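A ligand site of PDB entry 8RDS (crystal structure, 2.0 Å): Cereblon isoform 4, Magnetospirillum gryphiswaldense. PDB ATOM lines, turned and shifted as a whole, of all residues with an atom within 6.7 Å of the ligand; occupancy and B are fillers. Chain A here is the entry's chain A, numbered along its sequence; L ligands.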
ATOM      1  N   VAL A  49      36.136  12.421 -18.987  1.00  0.00           N
ATOM      2  CA  VAL A  49      35.190  12.676 -20.117  1.00  0.00           C
ATOM      3  C   VAL A  49      35.673  13.898 -20.901  1.00  0.00           C
ATOM      4  O   VAL A  49      36.495  14.668 -20.351  1.00  0.00           O
ATOM      5  CB  VAL A  49      33.751  12.859 -19.593  1.00  0.00           C
ATOM      6  CG1 VAL A  49      33.208  11.567 -19.004  1.00  0.00           C
ATOM      7  CG2 VAL A  49      33.652  14.003 -18.595  1.00  0.00           C
ATOM      8  N   PHE A  50      35.178  14.059 -22.119  1.00  0.00           N
ATOM      9  CA  PHE A  50      35.455  15.199 -23.028  1.00  0.00           C
ATOM     10  C   PHE A  50      34.133  15.763 -23.536  1.00  0.00           C
ATOM     11  O   PHE A  50      33.255  14.983 -23.920  1.00  0.00           O
ATOM     12  CB  PHE A  50      36.244  14.763 -24.264  1.00  0.00           C
ATOM     13  CG  PHE A  50      37.661  14.312 -24.028  1.00  0.00           C
ATOM     14  CD1 PHE A  50      38.685  15.240 -23.918  1.00  0.00           C
ATOM     15  CD2 PHE A  50      37.965  12.969 -23.952  1.00  0.00           C
ATOM     16  CE1 PHE A  50      39.994  14.825 -23.720  1.00  0.00           C
ATOM     17  CE2 PHE A  50      39.275  12.558 -23.768  1.00  0.00           C
ATOM     18  CZ  PHE A  50      40.291  13.481 -23.653  1.00  0.00           C
ATOM     19  N   ASN A  51      34.027  17.090 -23.589  1.00  0.00           N
ATOM     20  CA  ASN A  51      32.849  17.785 -24.156  1.00  0.00           C
ATOM     21  C   ASN A  51      33.097  18.016 -25.645  1.00  0.00           C
ATOM     22  O   ASN A  51      34.185  17.719 -26.162  1.00  0.00           O
ATOM     23  CB  ASN A  51      32.501  19.027 -23.342  1.00  0.00           C
ATOM     24  CG  ASN A  51      33.407  20.211 -23.594  1.00  0.00           C
ATOM     25  OD1 ASN A  51      34.368  20.145 -24.362  1.00  0.00           O
ATOM     26  ND2 ASN A  51      33.094  21.307 -22.931  1.00  0.00           N
ATOM     27  N   PRO A  52      32.093  18.522 -26.398  1.00  0.00           N
ATOM     28  CA  PRO A  52      32.253  18.770 -27.826  1.00  0.00           C
ATOM     29  C   PRO A  52      33.328  19.812 -28.166  1.00  0.00           C
ATOM     30  O   PRO A  52      33.751  19.835 -29.292  1.00  0.00           O
ATOM     31  CB  PRO A  52      30.868  19.271 -28.267  1.00  0.00           C
ATOM     32  CG  PRO A  52      29.919  18.745 -27.198  1.00  0.00           C
ATOM     33  CD  PRO A  52      30.727  18.812 -25.916  1.00  0.00           C
ATOM     34  N   ALA A  53      33.748  20.640 -27.211  1.00  0.00           N
ATOM     35  CA  ALA A  53      34.843  21.626 -27.373  1.00  0.00           C
ATOM     36  C   ALA A  53      36.200  20.963 -27.087  1.00  0.00           C
ATOM     37  O   ALA A  53      37.215  21.679 -27.126  1.00  0.00           O
ATOM     38  CB  ALA A  53      34.589  22.822 -26.494  1.00  0.00           C
ATOM     39  N   GLY A  54      36.207  19.654 -26.828  1.00  0.00           N
ATOM     40  CA  GLY A  54      37.422  18.833 -26.641  1.00  0.00           C
ATOM     41  C   GLY A  54      38.042  19.033 -25.267  1.00  0.00           C
ATOM     42  O   GLY A  54      39.164  18.553 -25.050  1.00  0.00           O
ATOM     43  N   MET A  55      37.366  19.735 -24.362  1.00  0.00           N
ATOM     44  CA  MET A  55      37.856  19.965 -22.987  1.00  0.00           C
ATOM     45  C   MET A  55      37.716  18.664 -22.202  1.00  0.00           C
ATOM     46  O   MET A  55      36.627  18.051 -22.249  1.00  0.00           O
ATOM     47  CB  MET A  55      37.058  21.071 -22.287  1.00  0.00           C
ATOM     48  CG  MET A  55      37.085  22.373 -23.053  1.00  0.00           C
ATOM     49  SD  MET A  55      36.230  23.664 -22.166  1.00  0.00           S
ATOM     50  CE  MET A  55      37.247  23.758 -20.691  1.00  0.00           C
ATOM     51  N   PHE A  57      37.520  16.665 -18.697  1.00  0.00           N
ATOM     52  CA  PHE A  57      37.108  16.863 -17.289  1.00  0.00           C
ATOM     53  C   PHE A  57      37.339  15.539 -16.570  1.00  0.00           C
ATOM     54  O   PHE A  57      36.916  14.485 -17.080  1.00  0.00           O
ATOM     55  CB  PHE A  57      35.656  17.329 -17.206  1.00  0.00           C
ATOM     56  CG  PHE A  57      35.343  18.590 -17.968  1.00  0.00           C
ATOM     57  CD1 PHE A  57      35.577  19.842 -17.425  1.00  0.00           C
ATOM     58  CD2 PHE A  57      34.796  18.527 -19.240  1.00  0.00           C
ATOM     59  CE1 PHE A  57      35.281  21.001 -18.135  1.00  0.00           C
ATOM     60  CE2 PHE A  57      34.480  19.677 -19.947  1.00  0.00           C
ATOM     61  CZ  PHE A  57      34.721  20.907 -19.393  1.00  0.00           C
ATOM     62  N   SER A  75      19.332  19.718 -19.901  1.00  0.00           N
ATOM     63  CA  SER A  75      19.511  19.294 -21.308  1.00  0.00           C
ATOM     64  C   SER A  75      20.063  17.872 -21.350  1.00  0.00           C
ATOM     65  O   SER A  75      20.866  17.533 -20.478  1.00  0.00           O
ATOM     66  CB  SER A  75      20.412  20.242 -22.055  1.00  0.00           C
ATOM     67  OG  SER A  75      20.603  19.776 -23.390  1.00  0.00           O
ATOM     68  N   GLU A  77      21.511  16.851 -24.253  1.00  0.00           N
ATOM     69  CA  GLU A  77      22.462  16.959 -25.398  1.00  0.00           C
ATOM     70  C   GLU A  77      23.883  16.664 -24.902  1.00  0.00           C
ATOM     71  O   GLU A  77      24.329  17.314 -23.940  1.00  0.00           O
ATOM     72  CB  GLU A  77      22.359  18.347 -26.034  1.00  0.00           C
ATOM     73  CG  GLU A  77      20.962  18.668 -26.551  1.00  0.00           C
ATOM     74  CD  GLU A  77      20.900  19.845 -27.520  1.00  0.00           C
ATOM     75  OE1 GLU A  77      21.624  20.837 -27.278  1.00  0.00           O
ATOM     76  OE2 GLU A  77      20.140  19.758 -28.511  1.00  0.00           O
ATOM     77  N   PHE A  78      24.527  15.661 -25.506  1.00  0.00           N
ATOM     78  CA  PHE A  78      25.925  15.233 -25.259  1.00  0.00           C
ATOM     79  C   PHE A  78      26.108  14.769 -23.810  1.00  0.00           C
ATOM     80  O   PHE A  78      27.242  14.844 -23.310  1.00  0.00           O
ATOM     81  CB  PHE A  78      26.923  16.366 -25.557  1.00  0.00           C
ATOM     82  CG  PHE A  78      26.839  16.941 -26.943  1.00  0.00           C
ATOM     83  CD1 PHE A  78      27.212  16.195 -28.046  1.00  0.00           C
ATOM     84  CD2 PHE A  78      26.371  18.235 -27.153  1.00  0.00           C
ATOM     85  CE1 PHE A  78      27.104  16.708 -29.332  1.00  0.00           C
ATOM     86  CE2 PHE A  78      26.263  18.748 -28.439  1.00  0.00           C
ATOM     87  CZ  PHE A  78      26.641  18.000 -29.521  1.00  0.00           C
ATOM     88  N   SER A  79      25.050  14.309 -23.144  1.00  0.00           N
ATOM     89  CA  SER A  79      25.138  13.780 -21.755  1.00  0.00           C
ATOM     90  C   SER A  79      26.130  12.608 -21.716  1.00  0.00           C
ATOM     91  O   SER A  79      26.010  11.713 -22.542  1.00  0.00           O
ATOM     92  CB  SER A  79      23.816  13.358 -21.214  1.00  0.00           C
ATOM     93  OG  SER A  79      23.976  12.902 -19.875  1.00  0.00           O
ATOM     94  N   TRP A  80      27.045  12.613 -20.750  1.00  0.00           N
ATOM     95  CA  TRP A  80      28.061  11.555 -20.546  1.00  0.00           C
ATOM     96  C   TRP A  80      27.428  10.325 -19.901  1.00  0.00           C
ATOM     97  O   TRP A  80      28.069   9.264 -19.937  1.00  0.00           O
ATOM     98  CB  TRP A  80      29.214  12.064 -19.688  1.00  0.00           C
ATOM     99  CG  TRP A  80      30.048  13.095 -20.387  1.00  0.00           C
ATOM    100  CD1 TRP A  80      30.562  13.017 -21.650  1.00  0.00           C
ATOM    101  CD2 TRP A  80      30.447  14.366 -19.853  1.00  0.00           C
ATOM    102  NE1 TRP A  80      31.266  14.161 -21.937  1.00  0.00           N
ATOM    103  CE2 TRP A  80      31.225  14.992 -20.850  1.00  0.00           C
ATOM    104  CE3 TRP A  80      30.237  15.021 -18.631  1.00  0.00           C
ATOM    105  CZ2 TRP A  80      31.768  16.258 -20.667  1.00  0.00           C
ATOM    106  CZ3 TRP A  80      30.798  16.261 -18.445  1.00  0.00           C
ATOM    107  CH2 TRP A  80      31.562  16.871 -19.454  1.00  0.00           C
ATOM    108  N   PHE A  81      26.244  10.467 -19.319  1.00  0.00           N
ATOM    109  CA  PHE A  81      25.587   9.437 -18.487  1.00  0.00           C
ATOM    110  C   PHE A  81      24.211   9.127 -19.090  1.00  0.00           C
ATOM    111  O   PHE A  81      23.331  10.008 -19.080  1.00  0.00           O
ATOM    112  CB  PHE A  81      25.510   9.933 -17.040  1.00  0.00           C
ATOM    113  CG  PHE A  81      26.836  10.261 -16.416  1.00  0.00           C
ATOM    114  CD1 PHE A  81      27.654   9.260 -15.905  1.00  0.00           C
ATOM    115  CD2 PHE A  81      27.269  11.577 -16.297  1.00  0.00           C
ATOM    116  CE1 PHE A  81      28.874   9.557 -15.312  1.00  0.00           C
ATOM    117  CE2 PHE A  81      28.489  11.874 -15.704  1.00  0.00           C
ATOM    118  CZ  PHE A  81      29.289  10.867 -15.204  1.00  0.00           C
ATOM    119  N   TYR A  84      20.339  10.491 -18.351  1.00  0.00           N
ATOM    120  CA  TYR A  84      20.399  11.710 -17.503  1.00  0.00           C
ATOM    121  C   TYR A  84      20.488  12.979 -18.358  1.00  0.00           C
ATOM    122  O   TYR A  84      21.252  13.005 -19.321  1.00  0.00           O
ATOM    123  CB  TYR A  84      21.562  11.667 -16.510  1.00  0.00           C
ATOM    124  CG  TYR A  84      21.476  10.550 -15.506  1.00  0.00           C
ATOM    125  CD1 TYR A  84      20.792  10.698 -14.316  1.00  0.00           C
ATOM    126  CD2 TYR A  84      22.074   9.329 -15.748  1.00  0.00           C
ATOM    127  CE1 TYR A  84      20.697   9.661 -13.404  1.00  0.00           C
ATOM    128  CE2 TYR A  84      22.015   8.288 -14.848  1.00  0.00           C
ATOM    129  CZ  TYR A  84      21.317   8.452 -13.663  1.00  0.00           C
ATOM    130  OH  TYR A  84      21.273   7.429 -12.764  1.00  0.00           O
ATOM    131  N   TRP A  86      21.510  17.125 -17.869  1.00  0.00           N
ATOM    132  CA  TRP A  86      22.465  17.889 -17.016  1.00  0.00           C
ATOM    133  C   TRP A  86      21.992  19.335 -16.910  1.00  0.00           C
ATOM    134  O   TRP A  86      21.310  19.814 -17.827  1.00  0.00           O
ATOM    135  CB  TRP A  86      23.896  17.829 -17.565  1.00  0.00           C
ATOM    136  CG  TRP A  86      23.985  18.151 -19.027  1.00  0.00           C
ATOM    137  CD1 TRP A  86      24.003  17.253 -20.051  1.00  0.00           C
ATOM    138  CD2 TRP A  86      24.051  19.452 -19.622  1.00  0.00           C
ATOM    139  NE1 TRP A  86      24.068  17.906 -21.246  1.00  0.00           N
ATOM    140  CE2 TRP A  86      24.102  19.257 -21.019  1.00  0.00           C
ATOM    141  CE3 TRP A  86      24.052  20.764 -19.130  1.00  0.00           C
ATOM    142  CZ2 TRP A  86      24.177  20.317 -21.921  1.00  0.00           C
ATOM    143  CZ3 TRP A  86      24.117  21.807 -20.022  1.00  0.00           C
ATOM    144  CH2 TRP A  86      24.187  21.593 -21.393  1.00  0.00           C
ATOM    145  N   THR A  87      22.315  19.970 -15.795  1.00  0.00           N
ATOM    146  CA  THR A  87      22.172  21.431 -15.568  1.00  0.00           C
ATOM    147  C   THR A  87      23.529  21.929 -15.078  1.00  0.00           C
ATOM    148  O   THR A  87      24.137  21.231 -14.237  1.00  0.00           O
ATOM    149  CB  THR A  87      21.055  21.728 -14.560  1.00  0.00           C
ATOM    150  OG1 THR A  87      19.823  21.226 -15.090  1.00  0.00           O
ATOM    151  CG2 THR A  87      20.878  23.210 -14.287  1.00  0.00           C
ATOM    152  N   ILE A  88      24.002  23.048 -15.617  1.00  0.00           N
ATOM    153  CA  ILE A  88      25.326  23.618 -15.238  1.00  0.00           C
ATOM    154  C   ILE A  88      25.250  23.988 -13.761  1.00  0.00           C
ATOM    155  O   ILE A  88      24.248  24.607 -13.340  1.00  0.00           O
ATOM    156  CB  ILE A  88      25.703  24.813 -16.140  1.00  0.00           C
ATOM    157  CG1 ILE A  88      26.062  24.347 -17.546  1.00  0.00           C
ATOM    158  CG2 ILE A  88      26.822  25.636 -15.513  1.00  0.00           C
ATOM    159  CD1 ILE A  88      25.909  25.411 -18.606  1.00  0.00           C
ATOM    160  N   HIS A  97      32.592  27.532 -12.445  1.00  0.00           N
ATOM    161  CA  HIS A  97      31.895  26.335 -12.962  1.00  0.00           C
ATOM    162  C   HIS A  97      32.460  25.070 -12.292  1.00  0.00           C
ATOM    163  O   HIS A  97      33.593  24.715 -12.621  1.00  0.00           O
ATOM    164  CB  HIS A  97      32.005  26.277 -14.483  1.00  0.00           C
ATOM    165  CG  HIS A  97      31.341  25.084 -15.061  1.00  0.00           C
ATOM    166  ND1 HIS A  97      31.777  24.499 -16.232  1.00  0.00           N
ATOM    167  CD2 HIS A  97      30.294  24.350 -14.637  1.00  0.00           C
ATOM    168  CE1 HIS A  97      30.995  23.477 -16.515  1.00  0.00           C
ATOM    169  NE2 HIS A  97      30.091  23.356 -15.550  1.00  0.00           N
ATOM    170  N   TRP A 100      28.120  19.737 -12.966  1.00  0.00           N
ATOM    171  CA  TRP A 100      26.730  19.579 -13.457  1.00  0.00           C
ATOM    172  C   TRP A 100      25.905  18.825 -12.420  1.00  0.00           C
ATOM    173  O   TRP A 100      26.449  17.929 -11.752  1.00  0.00           O
ATOM    174  CB  TRP A 100      26.712  18.880 -14.818  1.00  0.00           C
ATOM    175  CG  TRP A 100      27.602  19.527 -15.837  1.00  0.00           C
ATOM    176  CD1 TRP A 100      27.234  20.477 -16.738  1.00  0.00           C
ATOM    177  CD2 TRP A 100      29.013  19.314 -16.014  1.00  0.00           C
ATOM    178  NE1 TRP A 100      28.310  20.837 -17.490  1.00  0.00           N
ATOM    179  CE2 TRP A 100      29.415  20.159 -17.070  1.00  0.00           C
ATOM    180  CE3 TRP A 100      29.974  18.502 -15.398  1.00  0.00           C
ATOM    181  CZ2 TRP A 100      30.737  20.219 -17.509  1.00  0.00           C
ATOM    182  CZ3 TRP A 100      31.285  18.567 -15.829  1.00  0.00           C
ATOM    183  CH2 TRP A 100      31.656  19.408 -16.874  1.00  0.00           C
ATOM    184  N   TYR A 102      22.828  16.173 -12.503  1.00  0.00           N
ATOM    185  CA  TYR A 102      22.215  15.170 -13.405  1.00  0.00           C
ATOM    186  C   TYR A 102      20.877  14.744 -12.816  1.00  0.00           C
ATOM    187  O   TYR A 102      20.816  14.554 -11.592  1.00  0.00           O
ATOM    188  CB  TYR A 102      23.169  13.992 -13.612  1.00  0.00           C
ATOM    189  CG  TYR A 102      24.349  14.372 -14.465  1.00  0.00           C
ATOM    190  CD1 TYR A 102      24.262  14.335 -15.848  1.00  0.00           C
ATOM    191  CD2 TYR A 102      25.533  14.801 -13.890  1.00  0.00           C
ATOM    192  CE1 TYR A 102      25.336  14.703 -16.649  1.00  0.00           C
ATOM    193  CE2 TYR A 102      26.620  15.149 -14.672  1.00  0.00           C
ATOM    194  CZ  TYR A 102      26.521  15.117 -16.048  1.00  0.00           C
ATOM    195  OH  TYR A 102      27.579  15.496 -16.826  1.00  0.00           O
HETATM  196  C1  LIG L   1      27.517  19.525 -22.286  1.00  0.00           C
HETATM  197  C2  LIG L   1      27.725  21.180 -24.324  1.00  0.00           C
HETATM  198  C3  LIG L   1      26.415  20.912 -24.744  1.00  0.00           C
HETATM  199  C4  LIG L   1      26.624  22.488 -26.523  1.00  0.00           C
HETATM  200  C5  LIG L   1      30.706  22.932 -25.479  1.00  0.00           C
HETATM  201  O1  LIG L   1      27.168  15.484 -19.542  1.00  0.00           O
HETATM  202  N1  LIG L   1      29.517  20.595 -22.824  1.00  0.00           N
HETATM  203  C6  LIG L   1      28.423  18.868 -19.990  1.00  0.00           C
HETATM  204  O2  LIG L   1      29.529  17.199 -22.987  1.00  0.00           O
HETATM  205  C7  LIG L   1      25.873  21.563 -25.837  1.00  0.00           C
HETATM  206  C8  LIG L   1      27.910  22.774 -26.137  1.00  0.00           C
HETATM  207  C9  LIG L   1      28.483  22.125 -25.042  1.00  0.00           C
HETATM  208  C10 LIG L   1      28.880  17.418 -21.982  1.00  0.00           C
HETATM  209  N2  LIG L   1      28.284  16.393 -21.281  1.00  0.00           N
HETATM  210  C11 LIG L   1      28.640  18.845 -21.495  1.00  0.00           C
HETATM  211  C12 LIG L   1      27.395  17.847 -19.525  1.00  0.00           C
HETATM  212  C13 LIG L   1      27.592  16.482 -20.090  1.00  0.00           C
HETATM  213  O3  LIG L   1      29.818  19.690 -21.781  1.00  0.00           O
HETATM  214  C14 LIG L   1      28.288  20.471 -23.162  1.00  0.00           C
HETATM  215  O4  LIG L   1      29.747  22.355 -24.583  1.00  0.00           O
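A nitrogen (N2) of the ligand lies within hydrogen-bond range of the backbone carbonyl oxygen (O) of Phe 78 (2.8 Å).
N of Trp 80 is in hydrogen-bond range of O1 of the ligand, at 3.1 Å.
The side-chain hydroxyl (OH) of Tyr 102 lies within hydrogen-bond range of an oxygen (O1) of the ligand, 2.7 Å away.
The backbone NH of Ala 53 sits at hydrogen-bond distance from the side-chain amide oxygen of Asn 51.
The backbone NH (N) of Gly 54 sits at hydrogen-bond distance from the side-chain amide oxygen (OD1) of Asn 51, 3.1 Å away.
The backbone NH of Met 55 lies within hydrogen-bond range of the side-chain amide oxygen of Asn 51.
The backbone carbonyl oxygen (O) of Ser 75 lies within hydrogen-bond range of the backbone NH (N) of Trp 86, 2.7 Å away.
OG of Ser 79 lies within hydrogen-bond range of O of Tyr 84 (2.8 Å).
The side-chain hydroxyl (OG) of Ser 79 is in hydrogen-bond range of the backbone carbonyl oxygen (O) of Phe 81, at 3.1 Å.
The indole nitrogen (NE1) of Trp 86 is in hydrogen-bond range of the backbone carbonyl oxygen (O) of Glu 77, 2.8 Å away.
The backbone carbonyl oxygen (O) of Phe 50 sits at hydrogen-bond distance from the indole nitrogen (NE1) of Trp 80, 2.9 Å away.
Asn 51 touches the ligand.
CD of Pro 52 touches O2 of the ligand, 3.6 Å away.
Ser 79 touches the ligand.
Trp 86 touches the ligand (CZ2 to C1, 3.5 Å).
Trp 100 touches the ligand (NE1 to C6, 3.2 Å).
Hydrophobic or aromatic side chains that line the ligand: Pro 52, Phe 78, Trp 80, Trp 86, Trp 100 and Tyr 102.
Within 4 Å of the ligand: Asn 51, Pro 52, Phe 78, Ser 79, Trp 80, Trp 86, Trp 100 and Tyr 102.
Along chain A the residues within 4 Å of the ligand span positions 51 to 102.
The nearest printed residue that does not touch the ligand is Ala 53 (4.01 Å).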
